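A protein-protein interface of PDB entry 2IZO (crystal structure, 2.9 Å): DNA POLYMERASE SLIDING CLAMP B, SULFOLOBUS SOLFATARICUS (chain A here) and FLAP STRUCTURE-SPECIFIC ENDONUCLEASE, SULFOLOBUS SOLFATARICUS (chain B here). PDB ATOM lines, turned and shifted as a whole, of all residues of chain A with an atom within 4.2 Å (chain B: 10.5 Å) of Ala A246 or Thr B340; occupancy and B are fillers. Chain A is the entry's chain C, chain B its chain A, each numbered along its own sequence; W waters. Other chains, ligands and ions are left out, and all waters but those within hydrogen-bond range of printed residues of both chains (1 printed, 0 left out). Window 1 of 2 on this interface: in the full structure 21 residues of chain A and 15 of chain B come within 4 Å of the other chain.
O of Pro A247 sits at hydrogen-bond distance from NE2 of Gln B339, 3.2 Å away. The backbone NH of Thr B340 lies close to the backbone carbonyl oxygen of Pro A247 (3.1 Å). The side-chain amide oxygen (OE1) of Gln B339 sits at hydrogen-bond distance from the guanidinium group (NE) of Arg A248 (3.2 Å). The side-chain amide nitrogen (NE2) of Gln B339 sits at hydrogen-bond distance from the backbone carbonyl oxygen (O) of Ala A246 (2.8 Å).
The guanidinium group (NE) of Arg B344 sits close to the side-chain hydroxyl (OG1) of Thr B340. O of Val A45 is in hydrogen-bond range of N of Ala A246, 2.9 Å away.
Val A45 touches Gln B339 (CG1 to NE2, 3.5 Å). O of Val A45 touches CD2 of Leu B342 (3.8 Å). Ala A246 touches Thr B340. Ala A246 touches Leu B342 (CB to CD1, 3.8 Å). Pro A247 touches Trp B345 (CG to CH2, 3.7 Å). Gly B335 touches Arg A248. Arg B338 touches Arg A248 (O to CA, 3.4 Å).
No residue of chain B comes within 4 Å of Ile A245. Ala A246 touches three residues of chain B. Glu B15 touches none of the printed residues of chain A. Of the printed residues of chain A, Gly B335 touches Arg A248. Of the printed residues of chain A, Arg B338 touches Arg A248. Printed residues of chain A within 4 Å of Gln B339: Val A45 (3.5 Å), Ala A246 (2.8 Å), Pro A247 (3.2 Å) and Arg A248 (3.2 Å). Printed residues of chain A within 4 Å of Thr B340: Ala A246 (3.4 Å) and Pro A247 (3.0 Å). Printed residues of chain A within 4 Å of Leu B342: Val A45 and Ala A246. Arg B344 touches none of the printed residues of chain A. Printed residues of chain A within 4 Å of Trp B345: Pro A247. The nearest residue of chain B that does not touch Ala A246 is Gly B341 (4.2 Å). The nearest printed residue of chain A that does not touch Gly B335 is Pro A247 (7.7 Å).
Of the 18 printed residues of chain B, 6 touch a printed residue of chain A. Hydrophobic or aromatic side chains of chain B within 4 Å of the printed part of chain A: Leu B342 and Trp B345. Printed residues of chain A that touch a printed residue of chain B: Val A45, Ala A246, Pro A247 and Arg A248. Among the printed residues, no Asp or Glu carboxylate lies within 4 Å of a Lys or Arg side-chain nitrogen of the other chain.
Water W1 lies within hydrogen-bond range of the backbone carbonyl oxygen (O) of Ala A246 and the side-chain amide oxygen (OE1) of Gln B339.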
ATOM      1  N   VAL A  45       0.388 -12.682  -8.958  1.00  0.00           N
ATOM      2  CA  VAL A  45      -0.924 -12.158  -9.309  1.00  0.00           C
ATOM      3  C   VAL A  45      -0.815 -10.704  -9.742  1.00  0.00           C
ATOM      4  O   VAL A  45      -1.492 -10.275 -10.679  1.00  0.00           O
ATOM      5  CB  VAL A  45      -1.906 -12.268  -8.111  1.00  0.00           C
ATOM      6  CG1 VAL A  45      -3.243 -11.603  -8.424  1.00  0.00           C
ATOM      7  CG2 VAL A  45      -2.116 -13.717  -7.725  1.00  0.00           C
ATOM      8  N   TYR A 200     -11.423 -10.576 -11.949  1.00  0.00           N
ATOM      9  CA  TYR A 200     -10.212 -10.314 -11.165  1.00  0.00           C
ATOM     10  C   TYR A 200     -10.530 -10.278  -9.674  1.00  0.00           C
ATOM     11  O   TYR A 200     -11.671 -10.035  -9.282  1.00  0.00           O
ATOM     12  CB  TYR A 200      -9.567  -8.988 -11.587  1.00  0.00           C
ATOM     13  CG  TYR A 200      -9.270  -8.895 -13.062  1.00  0.00           C
ATOM     14  CD1 TYR A 200     -10.181  -8.317 -13.939  1.00  0.00           C
ATOM     15  CD2 TYR A 200      -8.081  -9.397 -13.584  1.00  0.00           C
ATOM     16  CE1 TYR A 200      -9.915  -8.235 -15.295  1.00  0.00           C
ATOM     17  CE2 TYR A 200      -7.806  -9.325 -14.945  1.00  0.00           C
ATOM     18  CZ  TYR A 200      -8.729  -8.743 -15.793  1.00  0.00           C
ATOM     19  OH  TYR A 200      -8.460  -8.665 -17.141  1.00  0.00           O
ATOM     20  N   ILE A 245      -2.719  -6.840 -13.372  1.00  0.00           N
ATOM     21  CA  ILE A 245      -3.468  -7.757 -12.502  1.00  0.00           C
ATOM     22  C   ILE A 245      -3.860  -9.012 -13.282  1.00  0.00           C
ATOM     23  O   ILE A 245      -4.448  -8.916 -14.361  1.00  0.00           O
ATOM     24  CB  ILE A 245      -4.747  -7.105 -11.908  1.00  0.00           C
ATOM     25  CG1 ILE A 245      -4.454  -5.700 -11.387  1.00  0.00           C
ATOM     26  CG2 ILE A 245      -5.326  -7.972 -10.799  1.00  0.00           C
ATOM     27  CD1 ILE A 245      -5.682  -4.900 -11.082  1.00  0.00           C
ATOM     28  N   ALA A 246      -3.531 -10.178 -12.723  1.00  0.00           N
ATOM     29  CA  ALA A 246      -3.823 -11.472 -13.347  1.00  0.00           C
ATOM     30  C   ALA A 246      -5.277 -11.891 -13.112  1.00  0.00           C
ATOM     31  O   ALA A 246      -5.769 -11.783 -11.988  1.00  0.00           O
ATOM     32  CB  ALA A 246      -2.865 -12.539 -12.823  1.00  0.00           C
ATOM     33  N   PRO A 247      -5.963 -12.378 -14.168  1.00  0.00           N
ATOM     34  CA  PRO A 247      -7.380 -12.762 -14.086  1.00  0.00           C
ATOM     35  C   PRO A 247      -7.673 -14.035 -13.286  1.00  0.00           C
ATOM     36  O   PRO A 247      -6.761 -14.790 -12.949  1.00  0.00           O
ATOM     37  CB  PRO A 247      -7.755 -12.992 -15.555  1.00  0.00           C
ATOM     38  CG  PRO A 247      -6.493 -13.428 -16.186  1.00  0.00           C
ATOM     39  CD  PRO A 247      -5.432 -12.587 -15.526  1.00  0.00           C
ATOM     40  N   ARG A 248      -8.951 -14.255 -12.988  1.00  0.00           N
ATOM     41  CA  ARG A 248      -9.409 -15.527 -12.438  1.00  0.00           C
ATOM     42  C   ARG A 248     -10.164 -16.310 -13.505  1.00  0.00           C
ATOM     43  O   ARG A 248     -10.839 -15.720 -14.348  1.00  0.00           O
ATOM     44  CB  ARG A 248     -10.260 -15.304 -11.190  1.00  0.00           C
ATOM     45  CG  ARG A 248      -9.409 -15.023  -9.972  1.00  0.00           C
ATOM     46  CD  ARG A 248     -10.225 -14.699  -8.751  1.00  0.00           C
ATOM     47  NE  ARG A 248      -9.358 -14.480  -7.598  1.00  0.00           N
ATOM     48  CZ  ARG A 248      -9.787 -14.327  -6.349  1.00  0.00           C
ATOM     49  NH1 ARG A 248     -11.086 -14.367  -6.072  1.00  0.00           N
ATOM     50  NH2 ARG A 248      -8.911 -14.136  -5.371  1.00  0.00           N
ATOM     51  N   SER B  14       2.219 -16.935   0.529  1.00  0.00           N
ATOM     52  CA  SER B  14       1.928 -16.242  -0.726  1.00  0.00           C
ATOM     53  C   SER B  14       1.987 -17.194  -1.921  1.00  0.00           C
ATOM     54  O   SER B  14       1.038 -17.271  -2.704  1.00  0.00           O
ATOM     55  CB  SER B  14       2.893 -15.070  -0.936  1.00  0.00           C
ATOM     56  OG  SER B  14       2.573 -13.980  -0.088  1.00  0.00           O
ATOM     57  N   GLU B  15       3.094 -17.925  -2.045  1.00  0.00           N
ATOM     58  CA  GLU B  15       3.282 -18.865  -3.148  1.00  0.00           C
ATOM     59  C   GLU B  15       2.366 -20.080  -3.019  1.00  0.00           C
ATOM     60  O   GLU B  15       2.056 -20.739  -4.010  1.00  0.00           O
ATOM     61  CB  GLU B  15       4.743 -19.298  -3.246  1.00  0.00           C
ATOM     62  N   LYS B  17      -0.748 -19.942  -1.743  1.00  0.00           N
ATOM     63  CA  LYS B  17      -2.134 -19.486  -1.874  1.00  0.00           C
ATOM     64  C   LYS B  17      -2.799 -20.004  -3.154  1.00  0.00           C
ATOM     65  O   LYS B  17      -2.240 -19.890  -4.246  1.00  0.00           O
ATOM     66  CB  LYS B  17      -2.183 -17.955  -1.825  1.00  0.00           C
ATOM     67  CG  LYS B  17      -3.571 -17.360  -1.646  1.00  0.00           C
ATOM     68  CD  LYS B  17      -3.516 -15.939  -1.086  1.00  0.00           C
ATOM     69  CE  LYS B  17      -3.225 -14.885  -2.157  1.00  0.00           C
ATOM     70  NZ  LYS B  17      -1.783 -14.809  -2.522  1.00  0.00           N
ATOM     71  N   GLY B  18      -3.992 -20.575  -2.998  1.00  0.00           N
ATOM     72  CA  GLY B  18      -4.756 -21.123  -4.117  1.00  0.00           C
ATOM     73  C   GLY B  18      -4.284 -22.494  -4.567  1.00  0.00           C
ATOM     74  O   GLY B  18      -4.406 -22.843  -5.743  1.00  0.00           O
ATOM     75  N   LYS B  19      -3.756 -23.276  -3.627  1.00  0.00           N
ATOM     76  CA  LYS B  19      -3.166 -24.577  -3.945  1.00  0.00           C
ATOM     77  C   LYS B  19      -3.756 -25.734  -3.144  1.00  0.00           C
ATOM     78  O   LYS B  19      -3.861 -25.676  -1.914  1.00  0.00           O
ATOM     79  CB  LYS B  19      -1.645 -24.537  -3.768  1.00  0.00           C
ATOM     80  CG  LYS B  19      -0.968 -23.471  -4.608  1.00  0.00           C
ATOM     81  CD  LYS B  19       0.519 -23.690  -4.706  1.00  0.00           C
ATOM     82  CE  LYS B  19       1.115 -22.933  -5.887  1.00  0.00           C
ATOM     83  NZ  LYS B  19       0.462 -23.258  -7.186  1.00  0.00           N
ATOM     84  N   LYS B 334     -11.613 -20.752  -2.107  1.00  0.00           N
ATOM     85  CA  LYS B 334     -12.155 -21.222  -3.384  1.00  0.00           C
ATOM     86  C   LYS B 334     -11.950 -20.170  -4.477  1.00  0.00           C
ATOM     87  O   LYS B 334     -11.773 -20.509  -5.649  1.00  0.00           O
ATOM     88  CB  LYS B 334     -13.639 -21.587  -3.248  1.00  0.00           C
ATOM     89  CG  LYS B 334     -14.180 -22.473  -4.377  1.00  0.00           C
ATOM     90  CD  LYS B 334     -15.626 -22.917  -4.131  1.00  0.00           C
ATOM     91  CE  LYS B 334     -15.727 -24.074  -3.129  1.00  0.00           C
ATOM     92  NZ  LYS B 334     -15.106 -25.341  -3.631  1.00  0.00           N
ATOM     93  N   GLY B 335     -11.972 -18.898  -4.079  1.00  0.00           N
ATOM     94  CA  GLY B 335     -11.638 -17.792  -4.971  1.00  0.00           C
ATOM     95  C   GLY B 335     -10.219 -17.895  -5.503  1.00  0.00           C
ATOM     96  O   GLY B 335      -9.999 -17.859  -6.717  1.00  0.00           O
ATOM     97  N   ALA B 336      -9.259 -18.048  -4.593  1.00  0.00           N
ATOM     98  CA  ALA B 336      -7.842 -18.147  -4.955  1.00  0.00           C
ATOM     99  C   ALA B 336      -7.536 -19.341  -5.863  1.00  0.00           C
ATOM    100  O   ALA B 336      -6.584 -19.305  -6.646  1.00  0.00           O
ATOM    101  CB  ALA B 336      -6.975 -18.186  -3.706  1.00  0.00           C
ATOM    102  N   SER B 337      -8.351 -20.388  -5.750  1.00  0.00           N
ATOM    103  CA  SER B 337      -8.237 -21.592  -6.579  1.00  0.00           C
ATOM    104  C   SER B 337      -8.359 -21.288  -8.075  1.00  0.00           C
ATOM    105  O   SER B 337      -7.734 -21.951  -8.903  1.00  0.00           O
ATOM    106  CB  SER B 337      -9.296 -22.616  -6.149  1.00  0.00           C
ATOM    107  OG  SER B 337      -9.760 -23.404  -7.235  1.00  0.00           O
ATOM    108  N   ARG B 338      -9.169 -20.281  -8.396  1.00  0.00           N
ATOM    109  CA  ARG B 338      -9.426 -19.865  -9.773  1.00  0.00           C
ATOM    110  C   ARG B 338      -8.349 -18.925 -10.319  1.00  0.00           C
ATOM    111  O   ARG B 338      -8.318 -18.643 -11.517  1.00  0.00           O
ATOM    112  CB  ARG B 338     -10.788 -19.168  -9.856  1.00  0.00           C
ATOM    113  CG  ARG B 338     -11.991 -20.057  -9.569  1.00  0.00           C
ATOM    114  CD  ARG B 338     -13.203 -19.241  -9.091  1.00  0.00           C
ATOM    115  NE  ARG B 338     -13.484 -18.072  -9.930  1.00  0.00           N
ATOM    116  CZ  ARG B 338     -14.125 -18.106 -11.098  1.00  0.00           C
ATOM    117  NH1 ARG B 338     -14.561 -19.257 -11.598  1.00  0.00           N
ATOM    118  NH2 ARG B 338     -14.328 -16.984 -11.775  1.00  0.00           N
ATOM    119  N   GLN B 339      -7.475 -18.450  -9.431  1.00  0.00           N
ATOM    120  CA  GLN B 339      -6.473 -17.433  -9.762  1.00  0.00           C
ATOM    121  C   GLN B 339      -5.388 -17.933 -10.705  1.00  0.00           C
ATOM    122  O   GLN B 339      -4.760 -18.965 -10.463  1.00  0.00           O
ATOM    123  CB  GLN B 339      -5.842 -16.852  -8.490  1.00  0.00           C
ATOM    124  CG  GLN B 339      -4.835 -15.724  -8.728  1.00  0.00           C
ATOM    125  CD  GLN B 339      -5.471 -14.438  -9.241  1.00  0.00           C
ATOM    126  OE1 GLN B 339      -6.378 -13.882  -8.617  1.00  0.00           O
ATOM    127  NE2 GLN B 339      -4.984 -13.954 -10.379  1.00  0.00           N
ATOM    128  N   THR B 340      -5.174 -17.181 -11.777  1.00  0.00           N
ATOM    129  CA  THR B 340      -4.125 -17.473 -12.734  1.00  0.00           C
ATOM    130  C   THR B 340      -2.836 -16.739 -12.349  1.00  0.00           C
ATOM    131  O   THR B 340      -2.865 -15.747 -11.616  1.00  0.00           O
ATOM    132  CB  THR B 340      -4.563 -17.083 -14.160  1.00  0.00           C
ATOM    133  OG1 THR B 340      -3.870 -17.890 -15.115  1.00  0.00           O
ATOM    134  CG2 THR B 340      -4.267 -15.630 -14.435  1.00  0.00           C
ATOM    135  N   GLY B 341      -1.706 -17.244 -12.834  1.00  0.00           N
ATOM    136  CA  GLY B 341      -0.423 -16.584 -12.633  1.00  0.00           C
ATOM    137  C   GLY B 341      -0.139 -15.618 -13.766  1.00  0.00           C
ATOM    138  O   GLY B 341      -0.413 -15.915 -14.932  1.00  0.00           O
ATOM    139  N   LEU B 342       0.414 -14.459 -13.422  1.00  0.00           N
ATOM    140  CA  LEU B 342       0.764 -13.440 -14.405  1.00  0.00           C
ATOM    141  C   LEU B 342       1.916 -13.920 -15.289  1.00  0.00           C
ATOM    142  O   LEU B 342       2.213 -13.316 -16.321  1.00  0.00           O
ATOM    143  CB  LEU B 342       1.139 -12.140 -13.686  1.00  0.00           C
ATOM    144  CG  LEU B 342       0.944 -10.775 -14.351  1.00  0.00           C
ATOM    145  CD1 LEU B 342      -0.439 -10.611 -14.963  1.00  0.00           C
ATOM    146  CD2 LEU B 342       1.188  -9.690 -13.326  1.00  0.00           C
ATOM    147  N   ASP B 343       2.539 -15.027 -14.882  1.00  0.00           N
ATOM    148  CA  ASP B 343       3.701 -15.580 -15.577  1.00  0.00           C
ATOM    149  C   ASP B 343       3.350 -16.566 -16.698  1.00  0.00           C
ATOM    150  O   ASP B 343       4.238 -17.218 -17.247  1.00  0.00           O
ATOM    151  CB  ASP B 343       4.698 -16.193 -14.576  1.00  0.00           C
ATOM    152  CG  ASP B 343       4.331 -17.609 -14.153  1.00  0.00           C
ATOM    153  OD1 ASP B 343       3.216 -17.830 -13.636  1.00  0.00           O
ATOM    154  OD2 ASP B 343       5.181 -18.508 -14.320  1.00  0.00           O
ATOM    155  N   ARG B 344       2.066 -16.672 -17.039  1.00  0.00           N
ATOM    156  CA  ARG B 344       1.661 -17.449 -18.212  1.00  0.00           C
ATOM    157  C   ARG B 344       1.442 -16.544 -19.427  1.00  0.00           C
ATOM    158  O   ARG B 344       0.850 -16.954 -20.426  1.00  0.00           O
ATOM    159  CB  ARG B 344       0.441 -18.336 -17.927  1.00  0.00           C
ATOM    160  CG  ARG B 344      -0.885 -17.608 -17.824  1.00  0.00           C
ATOM    161  CD  ARG B 344      -2.068 -18.549 -17.974  1.00  0.00           C
ATOM    162  NE  ARG B 344      -2.138 -19.514 -16.881  1.00  0.00           N
ATOM    163  CZ  ARG B 344      -3.175 -20.313 -16.640  1.00  0.00           C
ATOM    164  NH1 ARG B 344      -4.262 -20.262 -17.407  1.00  0.00           N
ATOM    165  NH2 ARG B 344      -3.128 -21.153 -15.613  1.00  0.00           N
ATOM    166  N   TRP B 345       1.933 -15.312 -19.328  1.00  0.00           N
ATOM    167  CA  TRP B 345       1.948 -14.383 -20.454  1.00  0.00           C
ATOM    168  C   TRP B 345       3.327 -13.734 -20.651  1.00  0.00           C
ATOM    169  O   TRP B 345       3.451 -12.735 -21.354  1.00  0.00           O
ATOM    170  CB  TRP B 345       0.846 -13.326 -20.301  1.00  0.00           C
ATOM    171  CG  TRP B 345      -0.541 -13.904 -20.417  1.00  0.00           C
ATOM    172  CD1 TRP B 345      -1.205 -14.227 -21.570  1.00  0.00           C
ATOM    173  CD2 TRP B 345      -1.427 -14.237 -19.342  1.00  0.00           C
ATOM    174  NE1 TRP B 345      -2.445 -14.738 -21.277  1.00  0.00           N
ATOM    175  CE2 TRP B 345      -2.607 -14.754 -19.917  1.00  0.00           C
ATOM    176  CE3 TRP B 345      -1.337 -14.146 -17.947  1.00  0.00           C
ATOM    177  CZ2 TRP B 345      -3.690 -15.180 -19.148  1.00  0.00           C
ATOM    178  CZ3 TRP B 345      -2.414 -14.569 -17.184  1.00  0.00           C
ATOM    179  CH2 TRP B 345      -3.576 -15.082 -17.789  1.00  0.00           C
ATOM    180  N   PHE B 346       4.358 -14.315 -20.037  1.00  0.00           N
ATOM    181  CA  PHE B 346       5.726 -13.835 -20.228  1.00  0.00           C
ATOM    182  C   PHE B 346       6.303 -14.392 -21.529  1.00  0.00           C
ATOM    183  O   PHE B 346       5.974 -13.923 -22.620  1.00  0.00           O
ATOM    184  CB  PHE B 346       6.639 -14.213 -19.049  1.00  0.00           C
ATOM    185  CG  PHE B 346       6.317 -13.507 -17.750  1.00  0.00           C
ATOM    186  CD1 PHE B 346       6.937 -13.914 -16.570  1.00  0.00           C
ATOM    187  CD2 PHE B 346       5.402 -12.457 -17.697  1.00  0.00           C
ATOM    188  CE1 PHE B 346       6.664 -13.282 -15.363  1.00  0.00           C
ATOM    189  CE2 PHE B 346       5.117 -11.825 -16.491  1.00  0.00           C
ATOM    190  CZ  PHE B 346       5.749 -12.243 -15.322  1.00  0.00           C
ATOM    191  OXT PHE B 346       7.104 -15.330 -21.527  1.00  0.00           O
HETATM  192  O   HOH W   1      -6.852 -10.956  -9.714  1.00  0.00           O
